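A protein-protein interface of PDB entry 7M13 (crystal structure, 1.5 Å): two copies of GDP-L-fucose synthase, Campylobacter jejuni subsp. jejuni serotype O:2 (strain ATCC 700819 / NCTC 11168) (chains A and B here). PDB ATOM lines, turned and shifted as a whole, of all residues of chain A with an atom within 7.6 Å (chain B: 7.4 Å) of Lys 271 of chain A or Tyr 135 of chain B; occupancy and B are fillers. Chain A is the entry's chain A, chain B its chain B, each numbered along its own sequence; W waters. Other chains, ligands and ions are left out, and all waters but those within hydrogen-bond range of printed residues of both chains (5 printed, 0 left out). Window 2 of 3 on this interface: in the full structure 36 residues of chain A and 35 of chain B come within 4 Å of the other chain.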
ATOM      1  N   GLU A 152       9.301  24.373 -23.070  1.00  0.00           N
ATOM      2  CA  GLU A 152       9.773  24.659 -24.448  1.00  0.00           C
ATOM      3  C   GLU A 152      10.041  23.356 -25.179  1.00  0.00           C
ATOM      4  O   GLU A 152       9.772  23.231 -26.410  1.00  0.00           O
ATOM      5  CB  GLU A 152      11.048  25.486 -24.368  1.00  0.00           C
ATOM      6  CG  GLU A 152      11.618  25.828 -25.734  1.00  0.00           C
ATOM      7  CD  GLU A 152      12.905  26.605 -25.562  1.00  0.00           C
ATOM      8  OE1 GLU A 152      13.904  25.991 -25.105  1.00  0.00           O
ATOM      9  OE2 GLU A 152      12.877  27.824 -25.771  1.00  0.00           O
ATOM     10  N   ILE A 156       8.532  22.039 -28.736  1.00  0.00           N
ATOM     11  CA  ILE A 156       9.382  21.728 -29.926  1.00  0.00           C
ATOM     12  C   ILE A 156       9.113  20.284 -30.391  1.00  0.00           C
ATOM     13  O   ILE A 156       8.877  20.030 -31.622  1.00  0.00           O
ATOM     14  CB  ILE A 156      10.865  22.008 -29.606  1.00  0.00           C
ATOM     15  CG1 ILE A 156      11.137  23.492 -29.406  1.00  0.00           C
ATOM     16  CG2 ILE A 156      11.744  21.418 -30.705  1.00  0.00           C
ATOM     17  CD1 ILE A 156      12.511  23.855 -28.845  1.00  0.00           C
ATOM     18  N   ILE A 267       8.789  31.765 -31.239  1.00  0.00           N
ATOM     19  CA  ILE A 267       9.889  30.890 -31.764  1.00  0.00           C
ATOM     20  C   ILE A 267      10.675  31.676 -32.814  1.00  0.00           C
ATOM     21  O   ILE A 267      10.070  32.557 -33.453  1.00  0.00           O
ATOM     22  CB  ILE A 267       9.357  29.533 -32.271  1.00  0.00           C
ATOM     23  CG1 ILE A 267      10.481  28.532 -32.571  1.00  0.00           C
ATOM     24  CG2 ILE A 267       8.427  29.701 -33.455  1.00  0.00           C
ATOM     25  CD1 ILE A 267      10.025  27.261 -33.283  1.00  0.00           C
ATOM     26  N   LYS A 271      17.680  27.816 -34.245  1.00  0.00           N
ATOM     27  CA  LYS A 271      18.218  27.285 -32.961  1.00  0.00           C
ATOM     28  C   LYS A 271      17.492  27.989 -31.805  1.00  0.00           C
ATOM     29  O   LYS A 271      18.164  28.633 -30.952  1.00  0.00           O
ATOM     30  CB  LYS A 271      19.741  27.449 -32.899  1.00  0.00           C
ATOM     31  CG  LYS A 271      20.522  26.581 -33.883  1.00  0.00           C
ATOM     32  CD  LYS A 271      21.750  25.908 -33.289  1.00  0.00           C
ATOM     33  CE  LYS A 271      22.667  26.861 -32.552  1.00  0.00           C
ATOM     34  NZ  LYS A 271      22.963  28.073 -33.355  1.00  0.00           N
ATOM     35  N   SER A 272      16.171  27.812 -31.762  1.00  0.00           N
ATOM     36  CA  SER A 272      15.222  28.559 -30.890  1.00  0.00           C
ATOM     37  C   SER A 272      15.291  28.108 -29.417  1.00  0.00           C
ATOM     38  O   SER A 272      15.192  26.901 -29.102  1.00  0.00           O
ATOM     39  CB  SER A 272      13.841  28.432 -31.383  1.00  0.00           C
ATOM     40  OG  SER A 272      12.971  29.045 -30.460  1.00  0.00           O
ATOM     41  N   LYS A 273      15.333  29.096 -28.536  1.00  0.00           N
ATOM     42  CA  LYS A 273      15.618  28.943 -27.096  1.00  0.00           C
ATOM     43  C   LYS A 273      15.176  30.240 -26.426  1.00  0.00           C
ATOM     44  O   LYS A 273      14.893  31.244 -27.131  1.00  0.00           O
ATOM     45  CB  LYS A 273      17.094  28.663 -26.822  1.00  0.00           C
ATOM     46  CG  LYS A 273      18.020  29.820 -27.123  1.00  0.00           C
ATOM     47  CD  LYS A 273      19.462  29.394 -27.267  1.00  0.00           C
ATOM     48  CE  LYS A 273      20.319  29.816 -26.098  1.00  0.00           C
ATOM     49  NZ  LYS A 273      21.695  29.277 -26.216  1.00  0.00           N
ATOM     50  N   ASN A 274      15.079  30.217 -25.102  1.00  0.00           N
ATOM     51  CA  ASN A 274      14.703  31.412 -24.287  1.00  0.00           C
ATOM     52  C   ASN A 274      13.350  31.923 -24.744  1.00  0.00           C
ATOM     53  O   ASN A 274      13.189  33.160 -24.937  1.00  0.00           O
ATOM     54  CB  ASN A 274      15.804  32.474 -24.332  1.00  0.00           C
ATOM     55  CG  ASN A 274      17.097  31.961 -23.740  1.00  0.00           C
ATOM     56  OD1 ASN A 274      17.075  31.276 -22.728  1.00  0.00           O
ATOM     57  ND2 ASN A 274      18.234  32.303 -24.335  1.00  0.00           N
ATOM     58  N   CYS B  72      21.204  10.959 -25.276  1.00  0.00           N
ATOM     59  CA  CYS B  72      21.064  11.967 -26.341  1.00  0.00           C
ATOM     60  C   CYS B  72      22.155  11.716 -27.383  1.00  0.00           C
ATOM     61  O   CYS B  72      23.347  11.842 -27.036  1.00  0.00           O
ATOM     62  CB  CYS B  72      21.197  13.355 -25.739  1.00  0.00           C
ATOM     63  SG  CYS B  72      20.969  14.689 -26.932  1.00  0.00           S
ATOM     64  N   VAL B  77      18.021  13.064 -31.700  1.00  0.00           N
ATOM     65  CA  VAL B  77      18.112  14.461 -31.189  1.00  0.00           C
ATOM     66  C   VAL B  77      16.723  15.109 -31.208  1.00  0.00           C
ATOM     67  O   VAL B  77      16.507  16.014 -30.412  1.00  0.00           O
ATOM     68  CB  VAL B  77      19.162  15.303 -31.946  1.00  0.00           C
ATOM     69  CG1 VAL B  77      18.699  15.683 -33.343  1.00  0.00           C
ATOM     70  CG2 VAL B  77      19.558  16.549 -31.164  1.00  0.00           C
ATOM     71  N   ARG B  80      13.544  15.936 -27.786  1.00  0.00           N
ATOM     72  CA  ARG B  80      13.999  17.012 -26.880  1.00  0.00           C
ATOM     73  C   ARG B  80      13.206  16.974 -25.573  1.00  0.00           C
ATOM     74  O   ARG B  80      13.770  17.184 -24.496  1.00  0.00           O
ATOM     75  CB  ARG B  80      13.780  18.357 -27.567  1.00  0.00           C
ATOM     76  CG  ARG B  80      14.575  19.490 -26.972  1.00  0.00           C
ATOM     77  CD  ARG B  80      14.533  20.687 -27.918  1.00  0.00           C
ATOM     78  NE  ARG B  80      15.385  21.795 -27.524  1.00  0.00           N
ATOM     79  CZ  ARG B  80      16.680  21.860 -27.759  1.00  0.00           C
ATOM     80  NH1 ARG B  80      17.295  20.867 -28.364  1.00  0.00           N
ATOM     81  NH2 ARG B  80      17.345  22.928 -27.407  1.00  0.00           N
ATOM     82  N   GLU B 117      28.797  25.073 -23.610  1.00  0.00           N
ATOM     83  CA  GLU B 117      29.380  24.704 -24.922  1.00  0.00           C
ATOM     84  C   GLU B 117      30.760  25.375 -25.062  1.00  0.00           C
ATOM     85  O   GLU B 117      31.692  24.716 -25.512  1.00  0.00           O
ATOM     86  CB  GLU B 117      28.411  25.174 -26.011  1.00  0.00           C
ATOM     87  CG  GLU B 117      28.911  24.923 -27.419  1.00  0.00           C
ATOM     88  CD  GLU B 117      27.837  25.125 -28.473  1.00  0.00           C
ATOM     89  OE1 GLU B 117      26.948  25.956 -28.249  1.00  0.00           O
ATOM     90  OE2 GLU B 117      27.917  24.459 -29.506  1.00  0.00           O
ATOM     91  N   ASP B 132      25.829  29.212 -21.904  1.00  0.00           N
ATOM     92  CA  ASP B 132      24.745  28.312 -22.378  1.00  0.00           C
ATOM     93  C   ASP B 132      25.319  26.971 -22.867  1.00  0.00           C
ATOM     94  O   ASP B 132      26.483  26.774 -23.144  1.00  0.00           O
ATOM     95  CB  ASP B 132      23.695  28.936 -23.305  1.00  0.00           C
ATOM     96  CG  ASP B 132      22.256  28.452 -23.037  1.00  0.00           C
ATOM     97  OD1 ASP B 132      21.387  29.219 -23.231  1.00  0.00           O
ATOM     98  OD2 ASP B 132      22.065  27.314 -22.590  1.00  0.00           O
ATOM     99  N   LEU B 133      24.408  26.027 -22.825  1.00  0.00           N
ATOM    100  CA  LEU B 133      24.669  24.641 -23.195  1.00  0.00           C
ATOM    101  C   LEU B 133      24.595  24.532 -24.724  1.00  0.00           C
ATOM    102  O   LEU B 133      23.958  25.404 -25.348  1.00  0.00           O
ATOM    103  CB  LEU B 133      23.604  23.759 -22.535  1.00  0.00           C
ATOM    104  CG  LEU B 133      23.480  23.816 -21.010  1.00  0.00           C
ATOM    105  CD1 LEU B 133      22.372  22.865 -20.591  1.00  0.00           C
ATOM    106  CD2 LEU B 133      24.791  23.451 -20.325  1.00  0.00           C
ATOM    107  N   GLU B 134      25.186  23.482 -25.253  1.00  0.00           N
ATOM    108  CA  GLU B 134      25.096  23.093 -26.693  1.00  0.00           C
ATOM    109  C   GLU B 134      23.624  22.859 -27.034  1.00  0.00           C
ATOM    110  O   GLU B 134      22.897  22.218 -26.248  1.00  0.00           O
ATOM    111  CB  GLU B 134      25.914  21.834 -26.964  1.00  0.00           C
ATOM    112  CG  GLU B 134      26.076  21.553 -28.450  1.00  0.00           C
ATOM    113  CD  GLU B 134      24.998  20.642 -29.016  1.00  0.00           C
ATOM    114  OE1 GLU B 134      24.565  20.883 -30.182  1.00  0.00           O
ATOM    115  OE2 GLU B 134      24.583  19.682 -28.289  1.00  0.00           O
ATOM    116  N   TYR B 135      23.175  23.362 -28.172  1.00  0.00           N
ATOM    117  CA  TYR B 135      21.743  23.380 -28.523  1.00  0.00           C
ATOM    118  C   TYR B 135      21.140  21.967 -28.585  1.00  0.00           C
ATOM    119  O   TYR B 135      20.049  21.707 -28.018  1.00  0.00           O
ATOM    120  CB  TYR B 135      21.548  24.095 -29.852  1.00  0.00           C
ATOM    121  CG  TYR B 135      20.092  24.248 -30.129  1.00  0.00           C
ATOM    122  CD1 TYR B 135      19.409  25.301 -29.563  1.00  0.00           C
ATOM    123  CD2 TYR B 135      19.388  23.298 -30.842  1.00  0.00           C
ATOM    124  CE1 TYR B 135      18.048  25.438 -29.721  1.00  0.00           C
ATOM    125  CE2 TYR B 135      18.012  23.418 -31.018  1.00  0.00           C
ATOM    126  CZ  TYR B 135      17.360  24.507 -30.460  1.00  0.00           C
ATOM    127  OH  TYR B 135      16.029  24.727 -30.596  1.00  0.00           O
ATOM    128  N   GLY B 136      21.772  21.033 -29.287  1.00  0.00           N
ATOM    129  CA  GLY B 136      21.187  19.702 -29.469  1.00  0.00           C
ATOM    130  C   GLY B 136      20.989  18.983 -28.145  1.00  0.00           C
ATOM    131  O   GLY B 136      19.959  18.271 -27.965  1.00  0.00           O
ATOM    132  N   ALA B 137      21.901  19.174 -27.209  1.00  0.00           N
ATOM    133  CA  ALA B 137      21.881  18.440 -25.925  1.00  0.00           C
ATOM    134  C   ALA B 137      21.364  19.357 -24.818  1.00  0.00           C
ATOM    135  O   ALA B 137      21.557  19.059 -23.638  1.00  0.00           O
ATOM    136  CB  ALA B 137      23.249  17.890 -25.624  1.00  0.00           C
ATOM    137  N   TYR B 138      20.687  20.439 -25.172  1.00  0.00           N
ATOM    138  CA  TYR B 138      20.285  21.468 -24.176  1.00  0.00           C
ATOM    139  C   TYR B 138      19.400  20.855 -23.093  1.00  0.00           C
ATOM    140  O   TYR B 138      19.596  21.081 -21.876  1.00  0.00           O
ATOM    141  CB  TYR B 138      19.551  22.569 -24.937  1.00  0.00           C
ATOM    142  CG  TYR B 138      18.992  23.731 -24.150  1.00  0.00           C
ATOM    143  CD1 TYR B 138      19.795  24.752 -23.646  1.00  0.00           C
ATOM    144  CD2 TYR B 138      17.624  23.824 -23.932  1.00  0.00           C
ATOM    145  CE1 TYR B 138      19.251  25.842 -22.978  1.00  0.00           C
ATOM    146  CE2 TYR B 138      17.068  24.919 -23.289  1.00  0.00           C
ATOM    147  CZ  TYR B 138      17.881  25.920 -22.802  1.00  0.00           C
ATOM    148  OH  TYR B 138      17.309  26.992 -22.169  1.00  0.00           O
ATOM    149  N   SER B 139      18.360  20.151 -23.494  1.00  0.00           N
ATOM    150  CA  SER B 139      17.394  19.586 -22.536  1.00  0.00           C
ATOM    151  C   SER B 139      17.994  18.413 -21.766  1.00  0.00           C
ATOM    152  O   SER B 139      17.734  18.281 -20.553  1.00  0.00           O
ATOM    153  CB  SER B 139      16.106  19.277 -23.199  1.00  0.00           C
ATOM    154  OG  SER B 139      16.216  18.183 -24.084  1.00  0.00           O
ATOM    155  N   PHE B 140      18.815  17.605 -22.410  1.00  0.00           N
ATOM    156  CA  PHE B 140      19.518  16.485 -21.746  1.00  0.00           C
ATOM    157  C   PHE B 140      20.506  17.034 -20.723  1.00  0.00           C
ATOM    158  O   PHE B 140      20.531  16.561 -19.574  1.00  0.00           O
ATOM    159  CB  PHE B 140      20.214  15.667 -22.824  1.00  0.00           C
ATOM    160  CG  PHE B 140      21.035  14.534 -22.288  1.00  0.00           C
ATOM    161  CD1 PHE B 140      20.480  13.301 -22.026  1.00  0.00           C
ATOM    162  CD2 PHE B 140      22.385  14.710 -22.071  1.00  0.00           C
ATOM    163  CE1 PHE B 140      21.262  12.267 -21.534  1.00  0.00           C
ATOM    164  CE2 PHE B 140      23.156  13.668 -21.596  1.00  0.00           C
ATOM    165  CZ  PHE B 140      22.593  12.464 -21.320  1.00  0.00           C
HETATM  166  O   HOH W   1      18.801  29.174 -22.315  1.00  0.00           O
HETATM  167  O   HOH W   2      15.986  25.442 -26.868  1.00  0.00           O
HETATM  168  O   HOH W   3      14.072  23.210 -25.401  1.00  0.00           O
HETATM  169  O   HOH W   4      15.082  27.895 -23.495  1.00  0.00           O
HETATM  170  O   HOH W   5      20.800  31.942 -22.779  1.00  0.00           O
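The side-chain hydroxyl (OH) of Tyr 135 of chain B sits at hydrogen-bond distance from the backbone carbonyl oxygen (O) of Ser 272 of chain A (2.8 Å).
The side-chain amino group of Lys 273 of chain A lies within salt-bridge range of the side-chain carboxylate of Asp 132 of chain B, at 3.0 Å.
The backbone carbonyl oxygen of Arg 80 of chain B sits at hydrogen-bond distance from the side-chain hydroxyl of Ser 139 of chain B (2.7 Å).
N of Glu 117 of chain B sits at hydrogen-bond distance from O of Asp 132 of chain B, 2.9 Å away.
The backbone carbonyl oxygen (O) of Tyr 135 of chain B lies within hydrogen-bond range of the guanidinium group (NH1) of Arg 80 of chain B.
OE2 of Glu 152 of chain A lies within hydrogen-bond range of N of Asn 274 of chain A (3.3 Å).
Among the printed residues, merely in contact across the chains: Lys 271 of chain A with Tyr 135 of chain B, Ile 156 of chain A with Arg 80 of chain B and Glu 152 of chain A with Tyr 138 of chain B.
Of the printed residues of chain B, Glu 152 of chain A touches Tyr 138 (3.8 Å).
Of the printed residues of chain B, Lys 273 of chain A touches Asp 132.
Of the printed residues of chain A, Arg 80 of chain B touches Ile 156 (3.8 Å).
Of the printed residues of chain A, Tyr 135 of chain B touches Lys 271 and Ser 272.
The nearest residue of chain A that does not touch Tyr 135 of chain B is Ile 156 of chain A (4.03 Å).
Of the 13 printed residues of chain B, 4 touch a printed residue of chain A.
Of the 7 printed residues of chain A, 5 touch a printed residue of chain B.
Among the printed residues, 5 pairs touch across the chains.
Among the printed residues, Asp or Glu carboxylates within 4 Å of a Lys or Arg side-chain nitrogen of the other chain: Lys 273 of chain A with Asp 132 of chain B.
No position is printed for both chains.
Of the 5 pairs that touch across the chains among the printed residues, none has its exchanged pair printed and touching as well.
Water W1 lies within hydrogen-bond range of the side-chain hydroxyl of Tyr 138 of chain B, the side-chain carboxylate of Asp 132 of chain B and the side-chain amide oxygen of Asn 274 of chain A.
Water W4 lies within hydrogen-bond range of OH of Tyr 138 of chain B, OE1 of Glu 152 of chain A and N of Asn 274 of chain A.
Water W2 lies within hydrogen-bond range of the side-chain carboxylate (OE1) of Glu 152 of chain A (2.8 Å), the backbone carbonyl oxygen (O) of Ser 272 of chain A (2.8 Å) and the guanidinium group (NH2) of Arg 80 of chain B (2.9 Å).
Water W3 bridges OE1 of Glu 152 of chain A (2.8 Å) and NE of Arg 80 of chain B (2.9 Å).
Water W5 lies within hydrogen-bond range of the side-chain carboxylate of Asp 132 of chain B (2.8 Å) and the side-chain amide nitrogen of Asn 274 of chain A (3.0 Å).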
